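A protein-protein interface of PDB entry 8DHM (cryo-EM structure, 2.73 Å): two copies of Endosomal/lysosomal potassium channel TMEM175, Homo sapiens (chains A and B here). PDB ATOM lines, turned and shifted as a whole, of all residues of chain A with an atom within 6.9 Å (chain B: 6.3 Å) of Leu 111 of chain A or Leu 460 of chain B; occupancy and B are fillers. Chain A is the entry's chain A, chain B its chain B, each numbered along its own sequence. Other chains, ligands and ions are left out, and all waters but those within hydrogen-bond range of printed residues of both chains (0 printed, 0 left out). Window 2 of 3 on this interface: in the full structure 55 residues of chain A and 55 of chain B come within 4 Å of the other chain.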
ATOM      1  N   MET A  36      10.391  22.975 -34.225  1.00  0.00           N
ATOM      2  CA  MET A  36       9.171  22.628 -33.514  1.00  0.00           C
ATOM      3  C   MET A  36       8.772  21.183 -33.777  1.00  0.00           C
ATOM      4  O   MET A  36       8.386  20.463 -32.846  1.00  0.00           O
ATOM      5  CB  MET A  36       8.069  23.606 -33.927  1.00  0.00           C
ATOM      6  CG  MET A  36       6.653  23.133 -33.756  1.00  0.00           C
ATOM      7  SD  MET A  36       5.496  24.466 -34.083  1.00  0.00           S
ATOM      8  CE  MET A  36       4.089  23.533 -34.650  1.00  0.00           C
ATOM      9  N   THR A 105       5.130  27.802 -39.504  1.00  0.00           N
ATOM     10  CA  THR A 105       4.578  27.933 -38.167  1.00  0.00           C
ATOM     11  C   THR A 105       4.588  29.390 -37.726  1.00  0.00           C
ATOM     12  O   THR A 105       5.196  30.258 -38.357  1.00  0.00           O
ATOM     13  CB  THR A 105       5.362  27.077 -37.160  1.00  0.00           C
ATOM     14  OG1 THR A 105       4.613  26.951 -35.946  1.00  0.00           O
ATOM     15  CG2 THR A 105       6.712  27.698 -36.842  1.00  0.00           C
ATOM     16  N   ASP A 106       3.890  29.641 -36.624  1.00  0.00           N
ATOM     17  CA  ASP A 106       3.937  30.920 -35.931  1.00  0.00           C
ATOM     18  C   ASP A 106       3.862  30.644 -34.433  1.00  0.00           C
ATOM     19  O   ASP A 106       3.946  29.495 -33.993  1.00  0.00           O
ATOM     20  CB  ASP A 106       2.827  31.852 -36.435  1.00  0.00           C
ATOM     21  CG  ASP A 106       1.441  31.440 -35.969  1.00  0.00           C
ATOM     22  OD1 ASP A 106       1.295  30.355 -35.372  1.00  0.00           O
ATOM     23  OD2 ASP A 106       0.490  32.212 -36.205  1.00  0.00           O
ATOM     24  N   ASP A 107       3.712  31.706 -33.643  1.00  0.00           N
ATOM     25  CA  ASP A 107       3.676  31.556 -32.194  1.00  0.00           C
ATOM     26  C   ASP A 107       2.435  30.795 -31.742  1.00  0.00           C
ATOM     27  O   ASP A 107       2.528  29.848 -30.947  1.00  0.00           O
ATOM     28  CB  ASP A 107       3.724  32.936 -31.543  1.00  0.00           C
ATOM     29  CG  ASP A 107       5.066  33.619 -31.728  1.00  0.00           C
ATOM     30  OD1 ASP A 107       6.087  32.910 -31.837  1.00  0.00           O
ATOM     31  OD2 ASP A 107       5.098  34.867 -31.770  1.00  0.00           O
ATOM     32  N   THR A 108       1.272  31.194 -32.253  1.00  0.00           N
ATOM     33  CA  THR A 108       0.025  30.536 -31.889  1.00  0.00           C
ATOM     34  C   THR A 108       0.041  29.065 -32.276  1.00  0.00           C
ATOM     35  O   THR A 108      -0.403  28.208 -31.502  1.00  0.00           O
ATOM     36  CB  THR A 108      -1.140  31.255 -32.566  1.00  0.00           C
ATOM     37  OG1 THR A 108      -1.029  32.664 -32.336  1.00  0.00           O
ATOM     38  CG2 THR A 108      -2.466  30.756 -32.032  1.00  0.00           C
ATOM     39  N   LEU A 109       0.534  28.753 -33.475  1.00  0.00           N
ATOM     40  CA  LEU A 109       0.580  27.364 -33.912  1.00  0.00           C
ATOM     41  C   LEU A 109       1.515  26.542 -33.038  1.00  0.00           C
ATOM     42  O   LEU A 109       1.215  25.391 -32.714  1.00  0.00           O
ATOM     43  CB  LEU A 109       1.008  27.282 -35.375  1.00  0.00           C
ATOM     44  CG  LEU A 109      -0.093  27.471 -36.418  1.00  0.00           C
ATOM     45  CD1 LEU A 109       0.469  27.322 -37.810  1.00  0.00           C
ATOM     46  CD2 LEU A 109      -1.217  26.492 -36.201  1.00  0.00           C
ATOM     47  N   ALA A 110       2.657  27.111 -32.653  1.00  0.00           N
ATOM     48  CA  ALA A 110       3.574  26.394 -31.776  1.00  0.00           C
ATOM     49  C   ALA A 110       2.949  26.116 -30.416  1.00  0.00           C
ATOM     50  O   ALA A 110       3.109  25.016 -29.872  1.00  0.00           O
ATOM     51  CB  ALA A 110       4.864  27.187 -31.617  1.00  0.00           C
ATOM     52  N   LEU A 111       2.233  27.087 -29.855  1.00  0.00           N
ATOM     53  CA  LEU A 111       1.570  26.854 -28.577  1.00  0.00           C
ATOM     54  C   LEU A 111       0.464  25.808 -28.691  1.00  0.00           C
ATOM     55  O   LEU A 111       0.322  24.944 -27.814  1.00  0.00           O
ATOM     56  CB  LEU A 111       1.030  28.177 -28.044  1.00  0.00           C
ATOM     57  CG  LEU A 111       2.145  29.196 -27.795  1.00  0.00           C
ATOM     58  CD1 LEU A 111       1.599  30.576 -27.553  1.00  0.00           C
ATOM     59  CD2 LEU A 111       3.006  28.765 -26.632  1.00  0.00           C
ATOM     60  N   LEU A 112      -0.322  25.854 -29.766  1.00  0.00           N
ATOM     61  CA  LEU A 112      -1.347  24.836 -29.955  1.00  0.00           C
ATOM     62  C   LEU A 112      -0.733  23.458 -30.176  1.00  0.00           C
ATOM     63  O   LEU A 112      -1.311  22.445 -29.766  1.00  0.00           O
ATOM     64  CB  LEU A 112      -2.251  25.213 -31.123  1.00  0.00           C
ATOM     65  CG  LEU A 112      -3.167  26.411 -30.891  1.00  0.00           C
ATOM     66  CD1 LEU A 112      -3.713  26.903 -32.207  1.00  0.00           C
ATOM     67  CD2 LEU A 112      -4.302  26.074 -29.944  1.00  0.00           C
ATOM     68  N   ASN A 113       0.431  23.396 -30.818  1.00  0.00           N
ATOM     69  CA  ASN A 113       1.136  22.130 -30.959  1.00  0.00           C
ATOM     70  C   ASN A 113       1.622  21.618 -29.609  1.00  0.00           C
ATOM     71  O   ASN A 113       1.621  20.408 -29.361  1.00  0.00           O
ATOM     72  CB  ASN A 113       2.305  22.293 -31.924  1.00  0.00           C
ATOM     73  CG  ASN A 113       3.109  21.031 -32.076  1.00  0.00           C
ATOM     74  OD1 ASN A 113       2.586  19.991 -32.466  1.00  0.00           O
ATOM     75  ND2 ASN A 113       4.382  21.105 -31.740  1.00  0.00           N
ATOM     76  N   LEU A 114       2.061  22.521 -28.732  1.00  0.00           N
ATOM     77  CA  LEU A 114       2.377  22.114 -27.367  1.00  0.00           C
ATOM     78  C   LEU A 114       1.159  21.514 -26.682  1.00  0.00           C
ATOM     79  O   LEU A 114       1.270  20.498 -25.985  1.00  0.00           O
ATOM     80  CB  LEU A 114       2.887  23.303 -26.555  1.00  0.00           C
ATOM     81  CG  LEU A 114       4.327  23.752 -26.765  1.00  0.00           C
ATOM     82  CD1 LEU A 114       4.511  25.149 -26.190  1.00  0.00           C
ATOM     83  CD2 LEU A 114       5.292  22.777 -26.140  1.00  0.00           C
ATOM     84  N   ALA A 115      -0.005  22.131 -26.872  1.00  0.00           N
ATOM     85  CA  ALA A 115      -1.241  21.577 -26.329  1.00  0.00           C
ATOM     86  C   ALA A 115      -1.524  20.183 -26.884  1.00  0.00           C
ATOM     87  O   ALA A 115      -1.915  19.273 -26.139  1.00  0.00           O
ATOM     88  CB  ALA A 115      -2.405  22.516 -26.634  1.00  0.00           C
ATOM     89  N   CYS A 116      -1.352  20.004 -28.194  1.00  0.00           N
ATOM     90  CA  CYS A 116      -1.585  18.698 -28.804  1.00  0.00           C
ATOM     91  C   CYS A 116      -0.625  17.647 -28.256  1.00  0.00           C
ATOM     92  O   CYS A 116      -1.019  16.498 -28.018  1.00  0.00           O
ATOM     93  CB  CYS A 116      -1.456  18.799 -30.322  1.00  0.00           C
ATOM     94  SG  CYS A 116      -1.360  17.204 -31.158  1.00  0.00           S
ATOM     95  N   VAL A 153      -7.782  19.602 -31.020  1.00  0.00           N
ATOM     96  CA  VAL A 153      -6.628  20.487 -31.148  1.00  0.00           C
ATOM     97  C   VAL A 153      -6.141  20.518 -32.593  1.00  0.00           C
ATOM     98  O   VAL A 153      -5.790  21.581 -33.123  1.00  0.00           O
ATOM     99  CB  VAL A 153      -5.507  20.072 -30.178  1.00  0.00           C
ATOM    100  CG1 VAL A 153      -4.363  21.050 -30.267  1.00  0.00           C
ATOM    101  CG2 VAL A 153      -6.013  20.027 -28.754  1.00  0.00           C
ATOM    102  N   GLY B 321       7.414  23.732 -21.420  1.00  0.00           N
ATOM    103  CA  GLY B 321       7.125  23.958 -22.821  1.00  0.00           C
ATOM    104  C   GLY B 321       7.139  25.418 -23.209  1.00  0.00           C
ATOM    105  O   GLY B 321       7.599  25.767 -24.296  1.00  0.00           O
ATOM    106  N   LEU B 322       6.645  26.293 -22.339  1.00  0.00           N
ATOM    107  CA  LEU B 322       6.692  27.717 -22.648  1.00  0.00           C
ATOM    108  C   LEU B 322       8.102  28.289 -22.548  1.00  0.00           C
ATOM    109  O   LEU B 322       8.457  29.197 -23.311  1.00  0.00           O
ATOM    110  CB  LEU B 322       5.744  28.473 -21.729  1.00  0.00           C
ATOM    111  CG  LEU B 322       4.267  28.348 -22.082  1.00  0.00           C
ATOM    112  CD1 LEU B 322       3.443  28.864 -20.940  1.00  0.00           C
ATOM    113  CD2 LEU B 322       3.924  29.070 -23.369  1.00  0.00           C
ATOM    114  N   PHE B 325       9.422  27.459 -25.700  1.00  0.00           N
ATOM    115  CA  PHE B 325       8.880  28.387 -26.685  1.00  0.00           C
ATOM    116  C   PHE B 325       9.700  29.670 -26.742  1.00  0.00           C
ATOM    117  O   PHE B 325      10.025  30.164 -27.828  1.00  0.00           O
ATOM    118  CB  PHE B 325       7.415  28.668 -26.347  1.00  0.00           C
ATOM    119  CG  PHE B 325       6.777  29.720 -27.196  1.00  0.00           C
ATOM    120  CD1 PHE B 325       6.295  29.416 -28.454  1.00  0.00           C
ATOM    121  CD2 PHE B 325       6.631  31.009 -26.724  1.00  0.00           C
ATOM    122  CE1 PHE B 325       5.705  30.383 -29.226  1.00  0.00           C
ATOM    123  CE2 PHE B 325       6.040  31.974 -27.497  1.00  0.00           C
ATOM    124  CZ  PHE B 325       5.577  31.661 -28.745  1.00  0.00           C
ATOM    125  N   VAL B 455       0.421  33.572 -17.278  1.00  0.00           N
ATOM    126  CA  VAL B 455       1.601  33.601 -18.140  1.00  0.00           C
ATOM    127  C   VAL B 455       1.322  32.945 -19.486  1.00  0.00           C
ATOM    128  O   VAL B 455       1.689  33.526 -20.519  1.00  0.00           O
ATOM    129  CB  VAL B 455       2.804  32.974 -17.408  1.00  0.00           C
ATOM    130  CG1 VAL B 455       3.943  32.692 -18.369  1.00  0.00           C
ATOM    131  CG2 VAL B 455       3.261  33.881 -16.284  1.00  0.00           C
ATOM    132  N   PRO B 456       0.704  31.765 -19.554  1.00  0.00           N
ATOM    133  CA  PRO B 456       0.323  31.231 -20.873  1.00  0.00           C
ATOM    134  C   PRO B 456      -0.532  32.186 -21.684  1.00  0.00           C
ATOM    135  O   PRO B 456      -0.245  32.423 -22.865  1.00  0.00           O
ATOM    136  CB  PRO B 456      -0.429  29.948 -20.511  1.00  0.00           C
ATOM    137  CG  PRO B 456       0.136  29.533 -19.215  1.00  0.00           C
ATOM    138  CD  PRO B 456       0.512  30.777 -18.480  1.00  0.00           C
ATOM    139  N   CYS B 457      -1.579  32.753 -21.081  1.00  0.00           N
ATOM    140  CA  CYS B 457      -2.440  33.668 -21.822  1.00  0.00           C
ATOM    141  C   CYS B 457      -1.654  34.851 -22.361  1.00  0.00           C
ATOM    142  O   CYS B 457      -1.835  35.241 -23.520  1.00  0.00           O
ATOM    143  CB  CYS B 457      -3.578  34.156 -20.930  1.00  0.00           C
ATOM    144  SG  CYS B 457      -4.747  32.876 -20.425  1.00  0.00           S
ATOM    145  N   ALA B 458      -0.772  35.424 -21.546  1.00  0.00           N
ATOM    146  CA  ALA B 458       0.059  36.532 -21.988  1.00  0.00           C
ATOM    147  C   ALA B 458       0.947  36.159 -23.165  1.00  0.00           C
ATOM    148  O   ALA B 458       1.363  37.049 -23.913  1.00  0.00           O
ATOM    149  CB  ALA B 458       0.918  37.030 -20.828  1.00  0.00           C
ATOM    150  N   PHE B 459       1.254  34.874 -23.342  1.00  0.00           N
ATOM    151  CA  PHE B 459       1.980  34.448 -24.531  1.00  0.00           C
ATOM    152  C   PHE B 459       1.076  34.385 -25.752  1.00  0.00           C
ATOM    153  O   PHE B 459       1.520  34.696 -26.861  1.00  0.00           O
ATOM    154  CB  PHE B 459       2.631  33.085 -24.298  1.00  0.00           C
ATOM    155  CG  PHE B 459       3.982  33.158 -23.657  1.00  0.00           C
ATOM    156  CD1 PHE B 459       5.056  33.699 -24.334  1.00  0.00           C
ATOM    157  CD2 PHE B 459       4.187  32.659 -22.385  1.00  0.00           C
ATOM    158  CE1 PHE B 459       6.296  33.758 -23.749  1.00  0.00           C
ATOM    159  CE2 PHE B 459       5.429  32.712 -21.802  1.00  0.00           C
ATOM    160  CZ  PHE B 459       6.483  33.264 -22.485  1.00  0.00           C
ATOM    161  N   LEU B 460      -0.185  33.989 -25.573  1.00  0.00           N
ATOM    162  CA  LEU B 460      -1.120  33.949 -26.687  1.00  0.00           C
ATOM    163  C   LEU B 460      -1.545  35.338 -27.132  1.00  0.00           C
ATOM    164  O   LEU B 460      -2.129  35.478 -28.210  1.00  0.00           O
ATOM    165  CB  LEU B 460      -2.368  33.142 -26.315  1.00  0.00           C
ATOM    166  CG  LEU B 460      -2.301  31.620 -26.422  1.00  0.00           C
ATOM    167  CD1 LEU B 460      -2.063  31.183 -27.864  1.00  0.00           C
ATOM    168  CD2 LEU B 460      -1.251  31.055 -25.482  1.00  0.00           C
ATOM    169  N   LEU B 461      -1.261  36.362 -26.327  1.00  0.00           N
ATOM    170  CA  LEU B 461      -1.662  37.730 -26.626  1.00  0.00           C
ATOM    171  C   LEU B 461      -0.485  38.689 -26.529  1.00  0.00           C
ATOM    172  O   LEU B 461      -0.687  39.895 -26.360  1.00  0.00           O
ATOM    173  CB  LEU B 461      -2.777  38.177 -25.681  1.00  0.00           C
ATOM    174  CG  LEU B 461      -3.961  37.226 -25.534  1.00  0.00           C
ATOM    175  CD1 LEU B 461      -4.796  37.644 -24.348  1.00  0.00           C
ATOM    176  CD2 LEU B 461      -4.794  37.192 -26.800  1.00  0.00           C
ATOM    177  N   LEU B 462       0.742  38.180 -26.634  1.00  0.00           N
ATOM    178  CA  LEU B 462       1.910  39.021 -26.415  1.00  0.00           C
ATOM    179  C   LEU B 462       2.014  40.110 -27.472  1.00  0.00           C
ATOM    180  O   LEU B 462       2.411  41.240 -27.169  1.00  0.00           O
ATOM    181  CB  LEU B 462       3.174  38.164 -26.389  1.00  0.00           C
ATOM    182  CG  LEU B 462       4.410  38.783 -25.741  1.00  0.00           C
ATOM    183  CD1 LEU B 462       4.074  39.380 -24.390  1.00  0.00           C
ATOM    184  CD2 LEU B 462       5.507  37.747 -25.595  1.00  0.00           C
ATOM    185  N   ARG B 463       1.677  39.792 -28.724  1.00  0.00           N
ATOM    186  CA  ARG B 463       1.602  40.830 -29.745  1.00  0.00           C
ATOM    187  C   ARG B 463       0.660  41.943 -29.305  1.00  0.00           C
ATOM    188  O   ARG B 463       1.020  43.127 -29.311  1.00  0.00           O
ATOM    189  CB  ARG B 463       1.128  40.227 -31.067  1.00  0.00           C
ATOM    190  CG  ARG B 463       2.027  39.149 -31.636  1.00  0.00           C
ATOM    191  CD  ARG B 463       3.348  39.713 -32.098  1.00  0.00           C
ATOM    192  NE  ARG B 463       4.220  38.675 -32.632  1.00  0.00           N
ATOM    193  CZ  ARG B 463       4.260  38.302 -33.903  1.00  0.00           C
ATOM    194  NH1 ARG B 463       3.478  38.858 -34.814  1.00  0.00           N
ATOM    195  NH2 ARG B 463       5.113  37.352 -34.272  1.00  0.00           N
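The guanidinium group (NH2) of Arg 463 of chain B is in salt-bridge range of the side-chain carboxylate (OD2) of Asp 107 of chain A (3.5 Å).
Phe 325 of chain B touches Asp 107 of chain A.
CD2 of Leu 111 of chain A touches CD2 of Leu 322 of chain B (3.4 Å).
Phe 325 of chain B touches Leu 111 of chain A (CD1 to CD2, 3.8 Å).
Leu 111 of chain A touches Leu 460 of chain B (CD1 to CD2, 3.6 Å).
Leu 114 of chain A touches Gly 321 of chain B (CD1 to O, 3.7 Å).
Of chain B, only Leu 322, Phe 325 and Leu 460 come within 4 Å of Leu 111 of chain A.
Of the printed residues of chain A, Leu 460 of chain B touches Leu 111 (3.6 Å).
Printed residues of chain B within 4 Å of Asp 107 of chain A: Phe 325 (3.4 Å) and Arg 463 (3.5 Å).
Printed residues of chain A within 4 Å of Arg 463 of chain B: Asp 107.
Of the printed residues of chain A, Gly 321 of chain B touches Leu 114.
Cys 116 of chain A touches none of the printed residues of chain B.
Cys 457 of chain B touches none of the printed residues of chain A.
The nearest residue of chain A that does not touch Leu 460 of chain B is Thr 108 of chain A (4.2 Å).
Of the 14 printed residues of chain A, 3 touch a printed residue of chain B.
Printed residues of chain A that touch a printed residue of chain B: Asp 107, Leu 111 and Leu 114.
Hydrophobic or aromatic side chains of chain A that line the printed part of chain B: Leu 111 and Leu 114.
Along chain A the printed residues that touch a printed residue of chain B span positions 107 to 114.
Among the printed residues, 6 pairs touch across the chains.
No position is printed for both chains.
Of the 6 pairs that touch across the chains among the printed residues, none has its exchanged pair printed and touching as well.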
